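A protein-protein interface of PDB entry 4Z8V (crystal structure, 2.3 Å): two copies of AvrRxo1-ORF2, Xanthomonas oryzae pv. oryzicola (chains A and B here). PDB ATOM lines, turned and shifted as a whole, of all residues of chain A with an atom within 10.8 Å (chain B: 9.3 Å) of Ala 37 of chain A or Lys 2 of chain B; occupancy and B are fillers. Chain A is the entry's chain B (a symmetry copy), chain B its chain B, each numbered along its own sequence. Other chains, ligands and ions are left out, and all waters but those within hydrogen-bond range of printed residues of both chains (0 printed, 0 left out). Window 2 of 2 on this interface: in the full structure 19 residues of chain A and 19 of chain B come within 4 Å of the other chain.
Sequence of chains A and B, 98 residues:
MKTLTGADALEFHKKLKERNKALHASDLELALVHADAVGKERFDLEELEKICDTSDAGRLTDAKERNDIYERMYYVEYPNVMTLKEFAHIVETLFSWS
The side-chain carboxylate of Asp 8 of chain B lies close to the backbone NH of Ala 37 of chain A, at 3.4 Å. The side-chain carboxylate (OD1) of Asp 36 of chain A lies close to the side-chain carboxylate (OD2) of Asp 8 of chain B, at 3.5 Å.
Among the printed residues, pairs that only touch across the chains: Leu 30 of chain A with Phe 12 of chain B (3.8 Å), Val 33 of chain A with Asp 8 of chain B (3.4 Å), Val 33 of chain A with Phe 12 of chain B (3.8 Å), His 34 of chain A with Met 1 of chain B (3.5 Å), Ala 37 of chain A with Lys 2 of chain B (3.3 Å) and Ala 37 of chain A with Leu 4 of chain B (3.7 Å).
Lys 2 of chain B touches just one residue of chain A: Ala 37 (3.3 Å). Of chain B, only Asp 8 (3.5 Å) comes within 4 Å of Asp 36 of chain A. No residue of chain B comes within 4 Å of Val 38 of chain A. Met 1 of chain B touches just one residue of chain A: His 34. No residue of chain A comes within 4 Å of Thr 3 of chain B. Of the printed residues of chain B, Val 33 of chain A touches Asp 8 and Phe 12. Printed residues of chain B within 4 Å of His 34 of chain A: Met 1 (3.5 Å). Of the printed residues of chain A, Asp 8 of chain B touches Val 33 (3.4 Å), Asp 36 (3.5 Å) and Ala 37 (3.3 Å). Of the printed residues of chain A, Phe 12 of chain B touches Leu 30 and Val 33. Printed residues of chain B within 4 Å of Leu 30 of chain A: Phe 12. The nearest residue of chain B that does not touch Ala 37 of chain A is Thr 3 of chain B (5.5 Å). The nearest printed residue of chain A that does not touch Asp 8 of chain B is Val 38 of chain A (5.7 Å).
Of the 18 printed residues of chain A, 5 touch a printed residue of chain B. Printed residues of chain A that touch a printed residue of chain B: Leu 30, Val 33, His 34, Asp 36 and Ala 37. Of the 10 printed residues of chain B, 5 touch a printed residue of chain A. Printed residues of chain B that touch a printed residue of chain A: Met 1, Lys 2, Leu 4, Asp 8 and Phe 12. Hydrophobic or aromatic side chains of chain B within 4 Å of the printed part of chain A: Met 1, Leu 4 and Phe 12. Among the printed residues, 8 pairs touch across the chains.
No position is printed for both chains.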
ATOM      1  N   GLU A  29      23.441 -14.212 -21.420  1.00  0.00           N
ATOM      2  CA  GLU A  29      22.564 -15.326 -21.030  1.00  0.00           C
ATOM      3  C   GLU A  29      22.007 -15.089 -19.633  1.00  0.00           C
ATOM      4  O   GLU A  29      20.794 -15.118 -19.418  1.00  0.00           O
ATOM      5  CB  GLU A  29      23.345 -16.649 -21.054  1.00  0.00           C
ATOM      6  CG  GLU A  29      23.634 -17.189 -22.456  1.00  0.00           C
ATOM      7  CD  GLU A  29      24.658 -18.328 -22.465  1.00  0.00           C
ATOM      8  OE1 GLU A  29      25.227 -18.657 -21.395  1.00  0.00           O
ATOM      9  OE2 GLU A  29      24.905 -18.885 -23.559  1.00  0.00           O
ATOM     10  N   LEU A  30      22.903 -14.829 -18.682  1.00  0.00           N
ATOM     11  CA  LEU A  30      22.487 -14.560 -17.318  1.00  0.00           C
ATOM     12  C   LEU A  30      21.601 -13.312 -17.207  1.00  0.00           C
ATOM     13  O   LEU A  30      20.586 -13.336 -16.502  1.00  0.00           O
ATOM     14  CB  LEU A  30      23.703 -14.457 -16.399  1.00  0.00           C
ATOM     15  CG  LEU A  30      24.440 -15.765 -16.129  1.00  0.00           C
ATOM     16  CD1 LEU A  30      25.666 -15.501 -15.266  1.00  0.00           C
ATOM     17  CD2 LEU A  30      23.510 -16.782 -15.458  1.00  0.00           C
ATOM     18  N   ALA A  31      21.958 -12.236 -17.906  1.00  0.00           N
ATOM     19  CA  ALA A  31      21.120 -11.018 -17.919  1.00  0.00           C
ATOM     20  C   ALA A  31      19.725 -11.260 -18.491  1.00  0.00           C
ATOM     21  O   ALA A  31      18.779 -10.597 -18.080  1.00  0.00           O
ATOM     22  CB  ALA A  31      21.793  -9.877 -18.683  1.00  0.00           C
ATOM     23  N   LEU A  32      19.593 -12.179 -19.451  1.00  0.00           N
ATOM     24  CA  LEU A  32      18.278 -12.444 -20.055  1.00  0.00           C
ATOM     25  C   LEU A  32      17.342 -13.180 -19.103  1.00  0.00           C
ATOM     26  O   LEU A  32      16.142 -12.892 -19.030  1.00  0.00           O
ATOM     27  CB  LEU A  32      18.416 -13.227 -21.363  1.00  0.00           C
ATOM     28  CG  LEU A  32      18.807 -12.434 -22.611  1.00  0.00           C
ATOM     29  CD1 LEU A  32      19.026 -13.381 -23.767  1.00  0.00           C
ATOM     30  CD2 LEU A  32      17.717 -11.445 -22.952  1.00  0.00           C
ATOM     31  N   VAL A  33      17.894 -14.134 -18.368  1.00  0.00           N
ATOM     32  CA  VAL A  33      17.112 -14.844 -17.369  1.00  0.00           C
ATOM     33  C   VAL A  33      16.612 -13.879 -16.305  1.00  0.00           C
ATOM     34  O   VAL A  33      15.433 -13.901 -15.944  1.00  0.00           O
ATOM     35  CB  VAL A  33      17.929 -15.958 -16.741  1.00  0.00           C
ATOM     36  CG1 VAL A  33      17.171 -16.579 -15.576  1.00  0.00           C
ATOM     37  CG2 VAL A  33      18.269 -16.998 -17.812  1.00  0.00           C
ATOM     38  N   HIS A  34      17.496 -13.010 -15.826  1.00  0.00           N
ATOM     39  CA  HIS A  34      17.113 -12.051 -14.800  1.00  0.00           C
ATOM     40  C   HIS A  34      16.100 -11.044 -15.350  1.00  0.00           C
ATOM     41  O   HIS A  34      15.234 -10.559 -14.616  1.00  0.00           O
ATOM     42  CB  HIS A  34      18.353 -11.329 -14.246  1.00  0.00           C
ATOM     43  CG  HIS A  34      18.039 -10.169 -13.349  1.00  0.00           C
ATOM     44  ND1 HIS A  34      17.837  -8.887 -13.825  1.00  0.00           N
ATOM     45  CD2 HIS A  34      17.904 -10.092 -12.000  1.00  0.00           C
ATOM     46  CE1 HIS A  34      17.582  -8.075 -12.814  1.00  0.00           C
ATOM     47  NE2 HIS A  34      17.615  -8.780 -11.698  1.00  0.00           N
ATOM     48  N   ALA A  35      16.215 -10.717 -16.638  1.00  0.00           N
ATOM     49  CA  ALA A  35      15.288  -9.769 -17.262  1.00  0.00           C
ATOM     50  C   ALA A  35      13.867 -10.347 -17.373  1.00  0.00           C
ATOM     51  O   ALA A  35      12.889  -9.640 -17.137  1.00  0.00           O
ATOM     52  CB  ALA A  35      15.802  -9.310 -18.621  1.00  0.00           C
ATOM     53  N   ASP A  36      13.759 -11.623 -17.737  1.00  0.00           N
ATOM     54  CA  ASP A  36      12.474 -12.324 -17.718  1.00  0.00           C
ATOM     55  C   ASP A  36      11.852 -12.304 -16.310  1.00  0.00           C
ATOM     56  O   ASP A  36      10.664 -12.052 -16.153  1.00  0.00           O
ATOM     57  CB  ASP A  36      12.659 -13.773 -18.197  1.00  0.00           C
ATOM     58  CG  ASP A  36      11.330 -14.531 -18.372  1.00  0.00           C
ATOM     59  OD1 ASP A  36      10.445 -14.447 -17.491  1.00  0.00           O
ATOM     60  OD2 ASP A  36      11.180 -15.229 -19.401  1.00  0.00           O
ATOM     61  N   ALA A  37      12.657 -12.573 -15.290  1.00  0.00           N
ATOM     62  CA  ALA A  37      12.154 -12.649 -13.921  1.00  0.00           C
ATOM     63  C   ALA A  37      11.608 -11.327 -13.381  1.00  0.00           C
ATOM     64  O   ALA A  37      10.666 -11.331 -12.590  1.00  0.00           O
ATOM     65  CB  ALA A  37      13.228 -13.187 -12.994  1.00  0.00           C
ATOM     66  N   VAL A  38      12.209 -10.204 -13.772  1.00  0.00           N
ATOM     67  CA  VAL A  38      11.737  -8.903 -13.292  1.00  0.00           C
ATOM     68  C   VAL A  38      10.705  -8.294 -14.236  1.00  0.00           C
ATOM     69  O   VAL A  38      10.181  -7.208 -13.976  1.00  0.00           O
ATOM     70  CB  VAL A  38      12.891  -7.874 -13.045  1.00  0.00           C
ATOM     71  CG1 VAL A  38      13.787  -8.303 -11.885  1.00  0.00           C
ATOM     72  CG2 VAL A  38      13.712  -7.650 -14.307  1.00  0.00           C
ATOM     73  N   GLY A  39      10.410  -8.985 -15.331  1.00  0.00           N
ATOM     74  CA  GLY A  39       9.478  -8.456 -16.311  1.00  0.00           C
ATOM     75  C   GLY A  39       9.992  -7.217 -17.036  1.00  0.00           C
ATOM     76  O   GLY A  39       9.237  -6.284 -17.315  1.00  0.00           O
ATOM     77  N   LYS A  40      11.286  -7.204 -17.337  1.00  0.00           N
ATOM     78  CA  LYS A  40      11.881  -6.141 -18.139  1.00  0.00           C
ATOM     79  C   LYS A  40      11.370  -6.258 -19.574  1.00  0.00           C
ATOM     80  O   LYS A  40      11.224  -7.369 -20.092  1.00  0.00           O
ATOM     81  CB  LYS A  40      13.407  -6.272 -18.083  1.00  0.00           C
ATOM     82  CG  LYS A  40      14.199  -5.162 -18.769  1.00  0.00           C
ATOM     83  CD  LYS A  40      15.678  -5.259 -18.390  1.00  0.00           C
ATOM     84  CE  LYS A  40      16.561  -4.603 -19.449  1.00  0.00           C
ATOM     85  NZ  LYS A  40      17.846  -4.106 -18.867  1.00  0.00           N
ATOM     86  N   GLU A  41      11.086  -5.125 -20.217  1.00  0.00           N
ATOM     87  CA  GLU A  41      10.517  -5.139 -21.569  1.00  0.00           C
ATOM     88  C   GLU A  41      11.454  -5.804 -22.574  1.00  0.00           C
ATOM     89  O   GLU A  41      12.661  -5.522 -22.578  1.00  0.00           O
ATOM     90  CB  GLU A  41      10.184  -3.717 -22.039  1.00  0.00           C
ATOM     91  CG  GLU A  41       9.797  -3.648 -23.512  1.00  0.00           C
ATOM     92  CD  GLU A  41       9.472  -2.240 -23.982  1.00  0.00           C
ATOM     93  OE1 GLU A  41       9.492  -1.309 -23.151  1.00  0.00           O
ATOM     94  OE2 GLU A  41       9.194  -2.069 -25.187  1.00  0.00           O
ATOM     95  N   ARG A  42      10.912  -6.688 -23.414  1.00  0.00           N
ATOM     96  CA  ARG A  42      11.722  -7.371 -24.424  1.00  0.00           C
ATOM     97  C   ARG A  42      12.413  -6.339 -25.317  1.00  0.00           C
ATOM     98  O   ARG A  42      11.824  -5.308 -25.662  1.00  0.00           O
ATOM     99  CB  ARG A  42      10.874  -8.332 -25.281  1.00  0.00           C
ATOM    100  CG  ARG A  42      11.718  -9.281 -26.163  1.00  0.00           C
ATOM    101  CD  ARG A  42      10.899 -10.008 -27.247  1.00  0.00           C
ATOM    102  NE  ARG A  42      10.234  -9.071 -28.157  1.00  0.00           N
ATOM    103  CZ  ARG A  42      10.700  -8.700 -29.351  1.00  0.00           C
ATOM    104  NH1 ARG A  42      11.847  -9.188 -29.814  1.00  0.00           N
ATOM    105  NH2 ARG A  42      10.013  -7.835 -30.090  1.00  0.00           N
ATOM    106  N   TYR A  75      20.572  -5.245 -21.928  1.00  0.00           N
ATOM    107  CA  TYR A  75      20.479  -6.305 -20.940  1.00  0.00           C
ATOM    108  C   TYR A  75      21.682  -6.398 -20.017  1.00  0.00           C
ATOM    109  O   TYR A  75      21.521  -6.573 -18.815  1.00  0.00           O
ATOM    110  CB  TYR A  75      20.290  -7.648 -21.640  1.00  0.00           C
ATOM    111  CG  TYR A  75      18.903  -7.817 -22.205  1.00  0.00           C
ATOM    112  CD1 TYR A  75      17.786  -7.788 -21.366  1.00  0.00           C
ATOM    113  CD2 TYR A  75      18.707  -8.018 -23.569  1.00  0.00           C
ATOM    114  CE1 TYR A  75      16.509  -7.949 -21.869  1.00  0.00           C
ATOM    115  CE2 TYR A  75      17.433  -8.187 -24.085  1.00  0.00           C
ATOM    116  CZ  TYR A  75      16.337  -8.154 -23.225  1.00  0.00           C
ATOM    117  OH  TYR A  75      15.066  -8.309 -23.714  1.00  0.00           O
ATOM    118  N   PRO A  79      20.890  -3.325 -16.411  1.00  0.00           N
ATOM    119  CA  PRO A  79      19.906  -4.306 -15.977  1.00  0.00           C
ATOM    120  C   PRO A  79      18.776  -3.721 -15.146  1.00  0.00           C
ATOM    121  O   PRO A  79      17.744  -4.301 -15.084  1.00  0.00           O
ATOM    122  CB  PRO A  79      20.736  -5.231 -15.137  1.00  0.00           C
ATOM    123  CG  PRO A  79      21.691  -4.396 -14.577  1.00  0.00           C
ATOM    124  CD  PRO A  79      22.085  -3.421 -15.589  1.00  0.00           C
ATOM    125  N   ASN A  80      18.960  -2.561 -14.554  1.00  0.00           N
ATOM    126  CA  ASN A  80      17.879  -1.919 -13.849  1.00  0.00           C
ATOM    127  C   ASN A  80      17.015  -1.004 -14.701  1.00  0.00           C
ATOM    128  O   ASN A  80      16.068  -0.475 -14.238  1.00  0.00           O
ATOM    129  CB  ASN A  80      18.395  -1.206 -12.617  1.00  0.00           C
ATOM    130  CG  ASN A  80      19.087  -2.133 -11.676  1.00  0.00           C
ATOM    131  OD1 ASN A  80      18.647  -3.245 -11.454  1.00  0.00           O
ATOM    132  ND2 ASN A  80      20.197  -1.696 -11.143  1.00  0.00           N
ATOM    133  N   MET A  82      14.165  -0.727 -17.263  1.00  0.00           N
ATOM    134  CA  MET A  82      13.130  -1.696 -17.541  1.00  0.00           C
ATOM    135  C   MET A  82      12.354  -1.503 -18.810  1.00  0.00           C
ATOM    136  O   MET A  82      11.660  -2.381 -19.216  1.00  0.00           O
ATOM    137  CB  MET A  82      12.186  -1.789 -16.376  1.00  0.00           C
ATOM    138  CG  MET A  82      12.861  -1.975 -15.073  1.00  0.00           C
ATOM    139  SD  MET A  82      13.343  -3.624 -14.770  1.00  0.00           S
ATOM    140  CE  MET A  82      11.910  -4.421 -15.232  1.00  0.00           C
ATOM    141  N   MET B   1      17.022  -7.857  -3.773  1.00  0.00           N
ATOM    142  CA  MET B   1      16.499  -7.915  -5.133  1.00  0.00           C
ATOM    143  C   MET B   1      15.450  -9.022  -5.242  1.00  0.00           C
ATOM    144  O   MET B   1      15.239  -9.803  -4.293  1.00  0.00           O
ATOM    145  CB  MET B   1      17.636  -8.129  -6.151  1.00  0.00           C
ATOM    146  CG  MET B   1      18.356  -9.482  -6.053  1.00  0.00           C
ATOM    147  SD  MET B   1      19.863  -9.604  -7.069  1.00  0.00           S
ATOM    148  CE  MET B   1      19.192  -9.805  -8.722  1.00  0.00           C
ATOM    149  N   LYS B   2      14.790  -9.086  -6.393  1.00  0.00           N
ATOM    150  CA  LYS B   2      13.735 -10.063  -6.592  1.00  0.00           C
ATOM    151  C   LYS B   2      14.285 -11.480  -6.577  1.00  0.00           C
ATOM    152  O   LYS B   2      15.312 -11.787  -7.194  1.00  0.00           O
ATOM    153  CB  LYS B   2      13.000  -9.804  -7.907  1.00  0.00           C
ATOM    154  CG  LYS B   2      11.690 -10.581  -8.031  1.00  0.00           C
ATOM    155  CD  LYS B   2      11.028 -10.401  -9.397  1.00  0.00           C
ATOM    156  CE  LYS B   2       9.592 -10.913  -9.363  1.00  0.00           C
ATOM    157  NZ  LYS B   2       9.495 -12.240  -8.674  1.00  0.00           N
ATOM    158  N   THR B   3      13.596 -12.341  -5.844  1.00  0.00           N
ATOM    159  CA  THR B   3      13.911 -13.764  -5.821  1.00  0.00           C
ATOM    160  C   THR B   3      13.529 -14.403  -7.159  1.00  0.00           C
ATOM    161  O   THR B   3      12.435 -14.169  -7.684  1.00  0.00           O
ATOM    162  CB  THR B   3      13.190 -14.462  -4.654  1.00  0.00           C
ATOM    163  OG1 THR B   3      13.648 -13.889  -3.418  1.00  0.00           O
ATOM    164  CG2 THR B   3      13.454 -15.970  -4.661  1.00  0.00           C
ATOM    165  N   LEU B   4      14.450 -15.184  -7.716  1.00  0.00           N
ATOM    166  CA  LEU B   4      14.188 -15.975  -8.924  1.00  0.00           C
ATOM    167  C   LEU B   4      13.551 -17.290  -8.476  1.00  0.00           C
ATOM    168  O   LEU B   4      14.028 -17.925  -7.524  1.00  0.00           O
ATOM    169  CB  LEU B   4      15.496 -16.275  -9.658  1.00  0.00           C
ATOM    170  CG  LEU B   4      16.082 -15.321 -10.704  1.00  0.00           C
ATOM    171  CD1 LEU B   4      15.813 -13.856 -10.412  1.00  0.00           C
ATOM    172  CD2 LEU B   4      17.590 -15.578 -10.860  1.00  0.00           C
ATOM    173  N   THR B   5      12.481 -17.702  -9.150  1.00  0.00           N
ATOM    174  CA  THR B   5      11.738 -18.895  -8.756  1.00  0.00           C
ATOM    175  C   THR B   5      11.531 -19.809  -9.961  1.00  0.00           C
ATOM    176  O   THR B   5      11.851 -19.422 -11.093  1.00  0.00           O
ATOM    177  CB  THR B   5      10.374 -18.507  -8.128  1.00  0.00           C
ATOM    178  OG1 THR B   5       9.568 -17.833  -9.100  1.00  0.00           O
ATOM    179  CG2 THR B   5      10.571 -17.557  -6.950  1.00  0.00           C
ATOM    180  N   GLY B   6      11.023 -21.013  -9.717  1.00  0.00           N
ATOM    181  CA  GLY B   6      10.625 -21.933 -10.771  1.00  0.00           C
ATOM    182  C   GLY B   6      11.635 -22.085 -11.886  1.00  0.00           C
ATOM    183  O   GLY B   6      12.805 -22.394 -11.650  1.00  0.00           O
ATOM    184  N   ALA B   7      11.184 -21.857 -13.113  1.00  0.00           N
ATOM    185  CA  ALA B   7      12.001 -22.112 -14.295  1.00  0.00           C
ATOM    186  C   ALA B   7      13.154 -21.116 -14.431  1.00  0.00           C
ATOM    187  O   ALA B   7      14.226 -21.471 -14.927  1.00  0.00           O
ATOM    188  CB  ALA B   7      11.128 -22.098 -15.549  1.00  0.00           C
ATOM    189  N   ASP B   8      12.931 -19.872 -14.015  1.00  0.00           N
ATOM    190  CA  ASP B   8      13.989 -18.861 -14.071  1.00  0.00           C
ATOM    191  C   ASP B   8      15.145 -19.199 -13.139  1.00  0.00           C
ATOM    192  O   ASP B   8      16.308 -19.097 -13.530  1.00  0.00           O
ATOM    193  CB  ASP B   8      13.440 -17.471 -13.743  1.00  0.00           C
ATOM    194  CG  ASP B   8      12.726 -16.829 -14.918  1.00  0.00           C
ATOM    195  OD1 ASP B   8      12.939 -17.284 -16.067  1.00  0.00           O
ATOM    196  OD2 ASP B   8      11.961 -15.860 -14.686  1.00  0.00           O
ATOM    197  N   ALA B   9      14.831 -19.607 -11.910  1.00  0.00           N
ATOM    198  CA  ALA B   9      15.869 -20.024 -10.970  1.00  0.00           C
ATOM    199  C   ALA B   9      16.680 -21.167 -11.556  1.00  0.00           C
ATOM    200  O   ALA B   9      17.919 -21.143 -11.506  1.00  0.00           O
ATOM    201  CB  ALA B   9      15.270 -20.439  -9.630  1.00  0.00           C
ATOM    202  N   PHE B  12      18.832 -19.915 -14.499  1.00  0.00           N
ATOM    203  CA  PHE B  12      19.944 -19.106 -14.023  1.00  0.00           C
ATOM    204  C   PHE B  12      20.992 -20.048 -13.461  1.00  0.00           C
ATOM    205  O   PHE B  12      22.182 -19.886 -13.683  1.00  0.00           O
ATOM    206  CB  PHE B  12      19.468 -18.147 -12.934  1.00  0.00           C
ATOM    207  CG  PHE B  12      20.465 -17.069 -12.598  1.00  0.00           C
ATOM    208  CD1 PHE B  12      20.455 -15.855 -13.282  1.00  0.00           C
ATOM    209  CD2 PHE B  12      21.410 -17.262 -11.607  1.00  0.00           C
ATOM    210  CE1 PHE B  12      21.372 -14.862 -12.993  1.00  0.00           C
ATOM    211  CE2 PHE B  12      22.329 -16.265 -11.303  1.00  0.00           C
ATOM    212  CZ  PHE B  12      22.307 -15.062 -12.001  1.00  0.00           C
